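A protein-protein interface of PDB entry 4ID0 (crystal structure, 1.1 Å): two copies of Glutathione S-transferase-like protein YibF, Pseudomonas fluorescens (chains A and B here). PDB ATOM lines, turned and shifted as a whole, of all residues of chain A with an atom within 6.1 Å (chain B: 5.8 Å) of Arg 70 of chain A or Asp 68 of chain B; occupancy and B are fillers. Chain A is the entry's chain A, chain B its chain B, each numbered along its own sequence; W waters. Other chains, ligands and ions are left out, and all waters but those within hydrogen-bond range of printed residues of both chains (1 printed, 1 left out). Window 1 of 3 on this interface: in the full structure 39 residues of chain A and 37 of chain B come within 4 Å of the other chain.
Water W1 bridges the backbone carbonyl oxygen (O) of Ala 101 of chain A (2.9 Å) and the side-chain carboxylate (OD2) of Asp 68 of chain B (3.5 Å).
Asp 68 of chain A touches Arg 70 of chain B, and with the chains exchanged Arg 70 of chain A touches Asp 68 of chain B.
Arg 70 of chain A touches its own counterpart, Arg 70 of chain B.
Positions printed for both chains: 67, 68, 69, 70, 71, 72 and 73.
Of the 9 pairs that touch across the chains among the printed residues, 3 have their exchanged pair printed and touching as well.
Hydrophobic or aromatic side chains of chain A within 4 Å of the printed part of chain B: Ala 101.
Of the 9 printed residues of chain B, 5 touch a printed residue of chain A.
Hydrophobic or aromatic side chains of chain B within 4 Å of the printed part of chain A: Leu 66, Tyr 67 and Val 71.
Among the printed residues, pairs that only touch across the chains: Arg 70 of chain A with Arg 70 of chain B, Leu 97 of chain A with Val 71 of chain B, Thr 98 of chain A with Leu 66 of chain B, Thr 98 of chain A with Val 71 of chain B, Ala 101 of chain A with Tyr 67 of chain B and Ala 101 of chain A with Asp 68 of chain B.
Of chain B, only Asp 68 and Arg 70 come within 4 Å of Arg 70 of chain A.
Printed residues of chain B within 4 Å of Leu 97 of chain A: Val 71 (3.7 Å).
Of the printed residues of chain B, Thr 98 of chain A touches Leu 66, Tyr 67 and Val 71.
Printed residues of chain A within 4 Å of Leu 66 of chain B: Thr 98 (3.5 Å).
Of the printed residues of chain A, Tyr 67 of chain B touches Thr 98 (3.5 Å) and Ala 101 (3.3 Å).
Printed residues of chain A within 4 Å of Asp 68 of chain B: Arg 70 (2.9 Å) and Ala 101 (3.6 Å).
The nearest printed residue of chain B that does not touch Leu 97 of chain A is Tyr 67 of chain B (4.4 Å).
The side-chain carboxylate (OD1) of Asp 68 of chain A sits close to the backbone NH (N) of Arg 70 of chain A, at 3.2 Å.
OD2 of Asp 104 of chain A is in salt-bridge range of NE of Arg 70 of chain A, 3.6 Å away.
The side-chain carboxylate of Asp 68 of chain B sits close to the backbone NH of Arg 70 of chain B.
OD2 of Asp 68 of chain A is in salt-bridge range of NH2 of Arg 70 of chain B (2.8 Å).
The guanidinium group (NH2) of Arg 70 of chain A lies within salt-bridge range of the side-chain carboxylate (OD2) of Asp 68 of chain B (2.9 Å).
The backbone carbonyl oxygen (O) of Tyr 67 of chain B is in hydrogen-bond range of the side-chain hydroxyl (OG1) of Thr 98 of chain A, at 3.5 Å.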
ATOM      1  N   LYS A  16       2.304   0.737  17.179  1.00  0.00           N
ATOM      2  CA  LYS A  16       2.157   1.647  16.026  1.00  0.00           C
ATOM      3  C   LYS A  16       2.459   0.916  14.728  1.00  0.00           C
ATOM      4  O   LYS A  16       1.771   1.121  13.708  1.00  0.00           O
ATOM      5  CB  LYS A  16       3.092   2.848  16.091  1.00  0.00           C
ATOM      6  CG  LYS A  16       2.865   3.822  17.234  1.00  0.00           C
ATOM      7  CD  LYS A  16       3.796   5.009  17.146  1.00  0.00           C
ATOM      8  CE  LYS A  16       5.253   4.630  17.429  1.00  0.00           C
ATOM      9  NZ  LYS A  16       6.200   5.714  17.117  1.00  0.00           N
ATOM     10  N   TYR A  67      15.375   0.135  12.610  1.00  0.00           N
ATOM     11  CA  TYR A  67      14.784   0.589  13.855  1.00  0.00           C
ATOM     12  C   TYR A  67      15.064   2.085  13.904  1.00  0.00           C
ATOM     13  O   TYR A  67      15.870   2.563  13.103  1.00  0.00           O
ATOM     14  CB  TYR A  67      15.371  -0.173  15.066  1.00  0.00           C
ATOM     15  CG  TYR A  67      16.882  -0.097  15.143  1.00  0.00           C
ATOM     16  CD1 TYR A  67      17.524   1.034  15.668  1.00  0.00           C
ATOM     17  CD2 TYR A  67      17.685  -1.147  14.711  1.00  0.00           C
ATOM     18  CE1 TYR A  67      18.873   1.112  15.717  1.00  0.00           C
ATOM     19  CE2 TYR A  67      19.083  -1.078  14.772  1.00  0.00           C
ATOM     20  CZ  TYR A  67      19.648   0.071  15.288  1.00  0.00           C
ATOM     21  OH  TYR A  67      21.022   0.276  15.368  1.00  0.00           O
ATOM     22  N   ASP A  68      14.442   2.879  14.789  1.00  0.00           N
ATOM     23  CA  ASP A  68      13.396   2.539  15.753  1.00  0.00           C
ATOM     24  C   ASP A  68      12.021   2.591  15.105  1.00  0.00           C
ATOM     25  O   ASP A  68      11.898   2.517  13.873  1.00  0.00           O
ATOM     26  CB  ASP A  68      13.523   3.491  16.932  1.00  0.00           C
ATOM     27  CG  ASP A  68      13.300   4.933  16.569  1.00  0.00           C
ATOM     28  OD1 ASP A  68      12.935   5.251  15.430  1.00  0.00           O
ATOM     29  OD2 ASP A  68      13.474   5.754  17.521  1.00  0.00           O
ATOM     30  N   SER A  69      10.953   2.661  15.901  1.00  0.00           N
ATOM     31  CA  SER A  69       9.623   2.571  15.323  1.00  0.00           C
ATOM     32  C   SER A  69       9.383   3.642  14.284  1.00  0.00           C
ATOM     33  O   SER A  69       8.683   3.356  13.310  1.00  0.00           O
ATOM     34  CB  SER A  69       8.540   2.649  16.405  1.00  0.00           C
ATOM     35  OG  SER A  69       8.474   3.937  17.027  1.00  0.00           O
ATOM     36  N   ARG A  70       9.901   4.862  14.457  1.00  0.00           N
ATOM     37  CA  ARG A  70       9.630   5.882  13.463  1.00  0.00           C
ATOM     38  C   ARG A  70      10.298   5.618  12.150  1.00  0.00           C
ATOM     39  O   ARG A  70       9.727   5.926  11.094  1.00  0.00           O
ATOM     40  CB  ARG A  70       9.998   7.266  13.990  1.00  0.00           C
ATOM     41  CG  ARG A  70       8.960   7.733  15.012  1.00  0.00           C
ATOM     42  CD  ARG A  70       8.973   9.207  15.251  1.00  0.00           C
ATOM     43  NE  ARG A  70       9.957   9.434  16.271  1.00  0.00           N
ATOM     44  CZ  ARG A  70      10.337  10.628  16.711  1.00  0.00           C
ATOM     45  NH1 ARG A  70       9.882  11.716  16.134  1.00  0.00           N
ATOM     46  NH2 ARG A  70      11.268  10.706  17.650  1.00  0.00           N
ATOM     47  N   VAL A  71      11.488   5.023  12.163  1.00  0.00           N
ATOM     48  CA  VAL A  71      12.158   4.618  10.923  1.00  0.00           C
ATOM     49  C   VAL A  71      11.363   3.502  10.241  1.00  0.00           C
ATOM     50  O   VAL A  71      11.170   3.520   9.023  1.00  0.00           O
ATOM     51  CB  VAL A  71      13.589   4.168  11.223  1.00  0.00           C
ATOM     52  CG1 VAL A  71      14.283   3.654   9.990  1.00  0.00           C
ATOM     53  CG2 VAL A  71      14.392   5.269  11.818  1.00  0.00           C
ATOM     54  N   ILE A  72      10.921   2.533  11.018  1.00  0.00           N
ATOM     55  CA  ILE A  72      10.135   1.403  10.484  1.00  0.00           C
ATOM     56  C   ILE A  72       8.839   1.903   9.875  1.00  0.00           C
ATOM     57  O   ILE A  72       8.450   1.433   8.795  1.00  0.00           O
ATOM     58  CB  ILE A  72       9.872   0.357  11.588  1.00  0.00           C
ATOM     59  CG1 ILE A  72      11.191  -0.271  12.067  1.00  0.00           C
ATOM     60  CG2 ILE A  72       8.877  -0.718  11.108  1.00  0.00           C
ATOM     61  CD1 ILE A  72      11.066  -1.012  13.349  1.00  0.00           C
ATOM     62  N   LEU A  73       8.141   2.834  10.555  1.00  0.00           N
ATOM     63  CA  LEU A  73       6.895   3.380  10.030  1.00  0.00           C
ATOM     64  C   LEU A  73       7.111   4.078   8.706  1.00  0.00           C
ATOM     65  O   LEU A  73       6.317   3.901   7.780  1.00  0.00           O
ATOM     66  CB  LEU A  73       6.271   4.320  11.074  1.00  0.00           C
ATOM     67  CG  LEU A  73       5.714   3.599  12.301  1.00  0.00           C
ATOM     68  CD1 LEU A  73       5.570   4.589  13.478  1.00  0.00           C
ATOM     69  CD2 LEU A  73       4.372   2.907  12.039  1.00  0.00           C
ATOM     70  N   ASP A  74       8.163   4.886   8.609  1.00  0.00           N
ATOM     71  CA  ASP A  74       8.491   5.550   7.353  1.00  0.00           C
ATOM     72  C   ASP A  74       8.751   4.491   6.251  1.00  0.00           C
ATOM     73  O   ASP A  74       8.162   4.528   5.171  1.00  0.00           O
ATOM     74  CB  ASP A  74       9.693   6.467   7.592  1.00  0.00           C
ATOM     75  CG  ASP A  74       9.958   7.393   6.423  1.00  0.00           C
ATOM     76  OD1 ASP A  74       9.390   8.500   6.353  1.00  0.00           O
ATOM     77  OD2 ASP A  74      10.718   7.001   5.545  1.00  0.00           O
ATOM     78  N   TYR A  75       9.608   3.523   6.533  1.00  0.00           N
ATOM     79  CA  TYR A  75       9.917   2.474   5.557  1.00  0.00           C
ATOM     80  C   TYR A  75       8.630   1.813   5.042  1.00  0.00           C
ATOM     81  O   TYR A  75       8.378   1.699   3.862  1.00  0.00           O
ATOM     82  CB  TYR A  75      10.850   1.427   6.189  1.00  0.00           C
ATOM     83  CG  TYR A  75      11.002   0.206   5.303  1.00  0.00           C
ATOM     84  CD1 TYR A  75      11.893   0.208   4.242  1.00  0.00           C
ATOM     85  CD2 TYR A  75      10.217  -0.939   5.499  1.00  0.00           C
ATOM     86  CE1 TYR A  75      12.001  -0.927   3.401  1.00  0.00           C
ATOM     87  CE2 TYR A  75      10.325  -2.033   4.682  1.00  0.00           C
ATOM     88  CZ  TYR A  75      11.201  -2.027   3.633  1.00  0.00           C
ATOM     89  OH  TYR A  75      11.275  -3.131   2.796  1.00  0.00           O
ATOM     90  N   ILE A  86       2.101   9.088   5.791  1.00  0.00           N
ATOM     91  CA  ILE A  86       2.970  10.190   6.108  1.00  0.00           C
ATOM     92  C   ILE A  86       2.991  11.092   4.873  1.00  0.00           C
ATOM     93  O   ILE A  86       3.419  10.655   3.831  1.00  0.00           O
ATOM     94  CB  ILE A  86       4.403   9.708   6.428  1.00  0.00           C
ATOM     95  CG1 ILE A  86       4.401   8.692   7.569  1.00  0.00           C
ATOM     96  CG2 ILE A  86       5.253  10.913   6.754  1.00  0.00           C
ATOM     97  CD1 ILE A  86       5.715   7.926   7.718  1.00  0.00           C
ATOM     98  N   LEU A  97       3.895  14.860  11.224  1.00  0.00           N
ATOM     99  CA  LEU A  97       5.021  14.304  11.944  1.00  0.00           C
ATOM    100  C   LEU A  97       5.189  14.907  13.318  1.00  0.00           C
ATOM    101  O   LEU A  97       5.662  14.196  14.214  1.00  0.00           O
ATOM    102  CB  LEU A  97       6.287  14.432  11.104  1.00  0.00           C
ATOM    103  CG  LEU A  97       6.350  13.445   9.912  1.00  0.00           C
ATOM    104  CD1 LEU A  97       7.597  13.798   9.080  1.00  0.00           C
ATOM    105  CD2 LEU A  97       6.412  12.006  10.414  1.00  0.00           C
ATOM    106  N   THR A  98       4.867  16.193  13.507  1.00  0.00           N
ATOM    107  CA  THR A  98       4.950  16.787  14.829  1.00  0.00           C
ATOM    108  C   THR A  98       3.868  16.213  15.744  1.00  0.00           C
ATOM    109  O   THR A  98       4.134  15.922  16.894  1.00  0.00           O
ATOM    110  CB  THR A  98       4.852  18.334  14.758  1.00  0.00           C
ATOM    111  OG1 THR A  98       5.973  18.850  14.038  1.00  0.00           O
ATOM    112  CG2 THR A  98       4.863  18.933  16.121  1.00  0.00           C
ATOM    113  N   ALA A 100       2.635  13.261  15.466  1.00  0.00           N
ATOM    114  CA  ALA A 100       3.174  11.938  15.815  1.00  0.00           C
ATOM    115  C   ALA A 100       4.231  12.023  16.909  1.00  0.00           C
ATOM    116  O   ALA A 100       4.256  11.155  17.810  1.00  0.00           O
ATOM    117  CB  ALA A 100       3.721  11.260  14.567  1.00  0.00           C
ATOM    118  N   ALA A 101       5.118  13.009  16.838  1.00  0.00           N
ATOM    119  CA  ALA A 101       6.163  13.183  17.843  1.00  0.00           C
ATOM    120  C   ALA A 101       5.515  13.544  19.165  1.00  0.00           C
ATOM    121  O   ALA A 101       6.028  13.117  20.220  1.00  0.00           O
ATOM    122  CB  ALA A 101       7.123  14.280  17.415  1.00  0.00           C
ATOM    123  N   ASP A 104       4.489  10.236  20.486  1.00  0.00           N
ATOM    124  CA  ASP A 104       5.661   9.500  20.953  1.00  0.00           C
ATOM    125  C   ASP A 104       6.149  10.068  22.258  1.00  0.00           C
ATOM    126  O   ASP A 104       6.597   9.303  23.127  1.00  0.00           O
ATOM    127  CB  ASP A 104       6.784   9.564  19.916  1.00  0.00           C
ATOM    128  CG  ASP A 104       6.551   8.617  18.785  1.00  0.00           C
ATOM    129  OD1 ASP A 104       6.216   7.450  19.072  1.00  0.00           O
ATOM    130  OD2 ASP A 104       6.667   8.948  17.590  1.00  0.00           O
ATOM    131  N   PRO B  56      15.339  20.295  21.036  1.00  0.00           N
ATOM    132  CA  PRO B  56      14.903  21.458  20.268  1.00  0.00           C
ATOM    133  C   PRO B  56      13.421  21.503  19.945  1.00  0.00           C
ATOM    134  O   PRO B  56      12.731  20.491  19.863  1.00  0.00           O
ATOM    135  CB  PRO B  56      15.692  21.296  18.957  1.00  0.00           C
ATOM    136  CG  PRO B  56      15.854  19.808  18.804  1.00  0.00           C
ATOM    137  CD  PRO B  56      16.091  19.347  20.209  1.00  0.00           C
ATOM    138  N   LEU B  66       7.466  22.943  15.225  1.00  0.00           N
ATOM    139  CA  LEU B  66       7.920  21.563  14.912  1.00  0.00           C
ATOM    140  C   LEU B  66       8.761  21.033  16.060  1.00  0.00           C
ATOM    141  O   LEU B  66       9.584  21.756  16.668  1.00  0.00           O
ATOM    142  CB  LEU B  66       8.763  21.539  13.638  1.00  0.00           C
ATOM    143  CG  LEU B  66       8.133  22.176  12.400  1.00  0.00           C
ATOM    144  CD1 LEU B  66       9.014  21.855  11.212  1.00  0.00           C
ATOM    145  CD2 LEU B  66       6.686  21.731  12.157  1.00  0.00           C
ATOM    146  N   TYR B  67       8.590  19.734  16.330  1.00  0.00           N
ATOM    147  CA  TYR B  67       9.432  18.973  17.250  1.00  0.00           C
ATOM    148  C   TYR B  67       9.126  17.513  16.904  1.00  0.00           C
ATOM    149  O   TYR B  67       8.153  17.226  16.199  1.00  0.00           O
ATOM    150  CB  TYR B  67       9.115  19.308  18.741  1.00  0.00           C
ATOM    151  CG  TYR B  67       7.649  19.238  19.084  1.00  0.00           C
ATOM    152  CD1 TYR B  67       7.062  18.039  19.462  1.00  0.00           C
ATOM    153  CD2 TYR B  67       6.841  20.356  19.004  1.00  0.00           C
ATOM    154  CE1 TYR B  67       5.695  17.959  19.768  1.00  0.00           C
ATOM    155  CE2 TYR B  67       5.496  20.304  19.338  1.00  0.00           C
ATOM    156  CZ  TYR B  67       4.918  19.073  19.674  1.00  0.00           C
ATOM    157  OH  TYR B  67       3.572  18.972  19.966  1.00  0.00           O
ATOM    158  N   ASP B  68       9.959  16.564  17.334  1.00  0.00           N
ATOM    159  CA  ASP B  68      11.246  16.700  18.030  1.00  0.00           C
ATOM    160  C   ASP B  68      12.388  16.871  17.010  1.00  0.00           C
ATOM    161  O   ASP B  68      12.166  17.290  15.867  1.00  0.00           O
ATOM    162  CB  ASP B  68      11.445  15.487  18.943  1.00  0.00           C
ATOM    163  CG  ASP B  68      11.670  14.210  18.195  1.00  0.00           C
ATOM    164  OD1 ASP B  68      11.501  14.189  16.971  1.00  0.00           O
ATOM    165  OD2 ASP B  68      12.019  13.203  18.847  1.00  0.00           O
ATOM    166  N   SER B  69      13.622  16.617  17.455  1.00  0.00           N
ATOM    167  CA  SER B  69      14.765  16.894  16.591  1.00  0.00           C
ATOM    168  C   SER B  69      14.676  16.220  15.245  1.00  0.00           C
ATOM    169  O   SER B  69      15.091  16.827  14.260  1.00  0.00           O
ATOM    170  CB  SER B  69      16.077  16.522  17.266  1.00  0.00           C
ATOM    171  OG  SER B  69      16.215  15.122  17.470  1.00  0.00           O
ATOM    172  N   ARG B  70      14.183  14.978  15.157  1.00  0.00           N
ATOM    173  CA  ARG B  70      14.212  14.365  13.840  1.00  0.00           C
ATOM    174  C   ARG B  70      13.238  15.030  12.888  1.00  0.00           C
ATOM    175  O   ARG B  70      13.525  15.052  11.671  1.00  0.00           O
ATOM    176  CB  ARG B  70      13.907  12.898  13.927  1.00  0.00           C
ATOM    177  CG  ARG B  70      14.863  12.104  14.685  1.00  0.00           C
ATOM    178  CD  ARG B  70      14.538  10.649  14.473  1.00  0.00           C
ATOM    179  NE  ARG B  70      15.047   9.813  15.563  1.00  0.00           N
ATOM    180  CZ  ARG B  70      14.639   8.561  15.793  1.00  0.00           C
ATOM    181  NH1 ARG B  70      13.737   7.951  14.918  1.00  0.00           N
ATOM    182  NH2 ARG B  70      15.166   7.899  16.856  1.00  0.00           N
ATOM    183  N   VAL B  71      12.110  15.533  13.364  1.00  0.00           N
ATOM    184  CA  VAL B  71      11.158  16.243  12.518  1.00  0.00           C
ATOM    185  C   VAL B  71      11.790  17.570  12.056  1.00  0.00           C
ATOM    186  O   VAL B  71      11.658  17.957  10.879  1.00  0.00           O
ATOM    187  CB  VAL B  71       9.865  16.478  13.279  1.00  0.00           C
ATOM    188  CG1 VAL B  71       8.887  17.302  12.453  1.00  0.00           C
ATOM    189  CG2 VAL B  71       9.241  15.162  13.759  1.00  0.00           C
ATOM    190  N   ILE B  72      12.435  18.270  12.967  1.00  0.00           N
ATOM    191  CA  ILE B  72      13.106  19.524  12.625  1.00  0.00           C
ATOM    192  C   ILE B  72      14.195  19.307  11.591  1.00  0.00           C
ATOM    193  O   ILE B  72      14.342  20.096  10.645  1.00  0.00           O
ATOM    194  CB  ILE B  72      13.661  20.179  13.894  1.00  0.00           C
ATOM    195  CG1 ILE B  72      12.536  20.565  14.858  1.00  0.00           C
ATOM    196  CG2 ILE B  72      14.581  21.374  13.607  1.00  0.00           C
ATOM    197  CD1 ILE B  72      12.929  20.904  16.275  1.00  0.00           C
ATOM    198  N   LEU B  73      14.988  18.260  11.767  1.00  0.00           N
ATOM    199  CA  LEU B  73      16.073  17.975  10.824  1.00  0.00           C
ATOM    200  C   LEU B  73      15.517  17.675   9.452  1.00  0.00           C
ATOM    201  O   LEU B  73      16.066  18.160   8.437  1.00  0.00           O
ATOM    202  CB  LEU B  73      16.884  16.784  11.330  1.00  0.00           C
ATOM    203  CG  LEU B  73      17.749  17.100  12.560  1.00  0.00           C
ATOM    204  CD1 LEU B  73      18.142  15.832  13.310  1.00  0.00           C
ATOM    205  CD2 LEU B  73      19.001  17.897  12.174  1.00  0.00           C
HETATM  206  O   HOH W   1       8.911  13.037  20.403  1.00  0.00           O
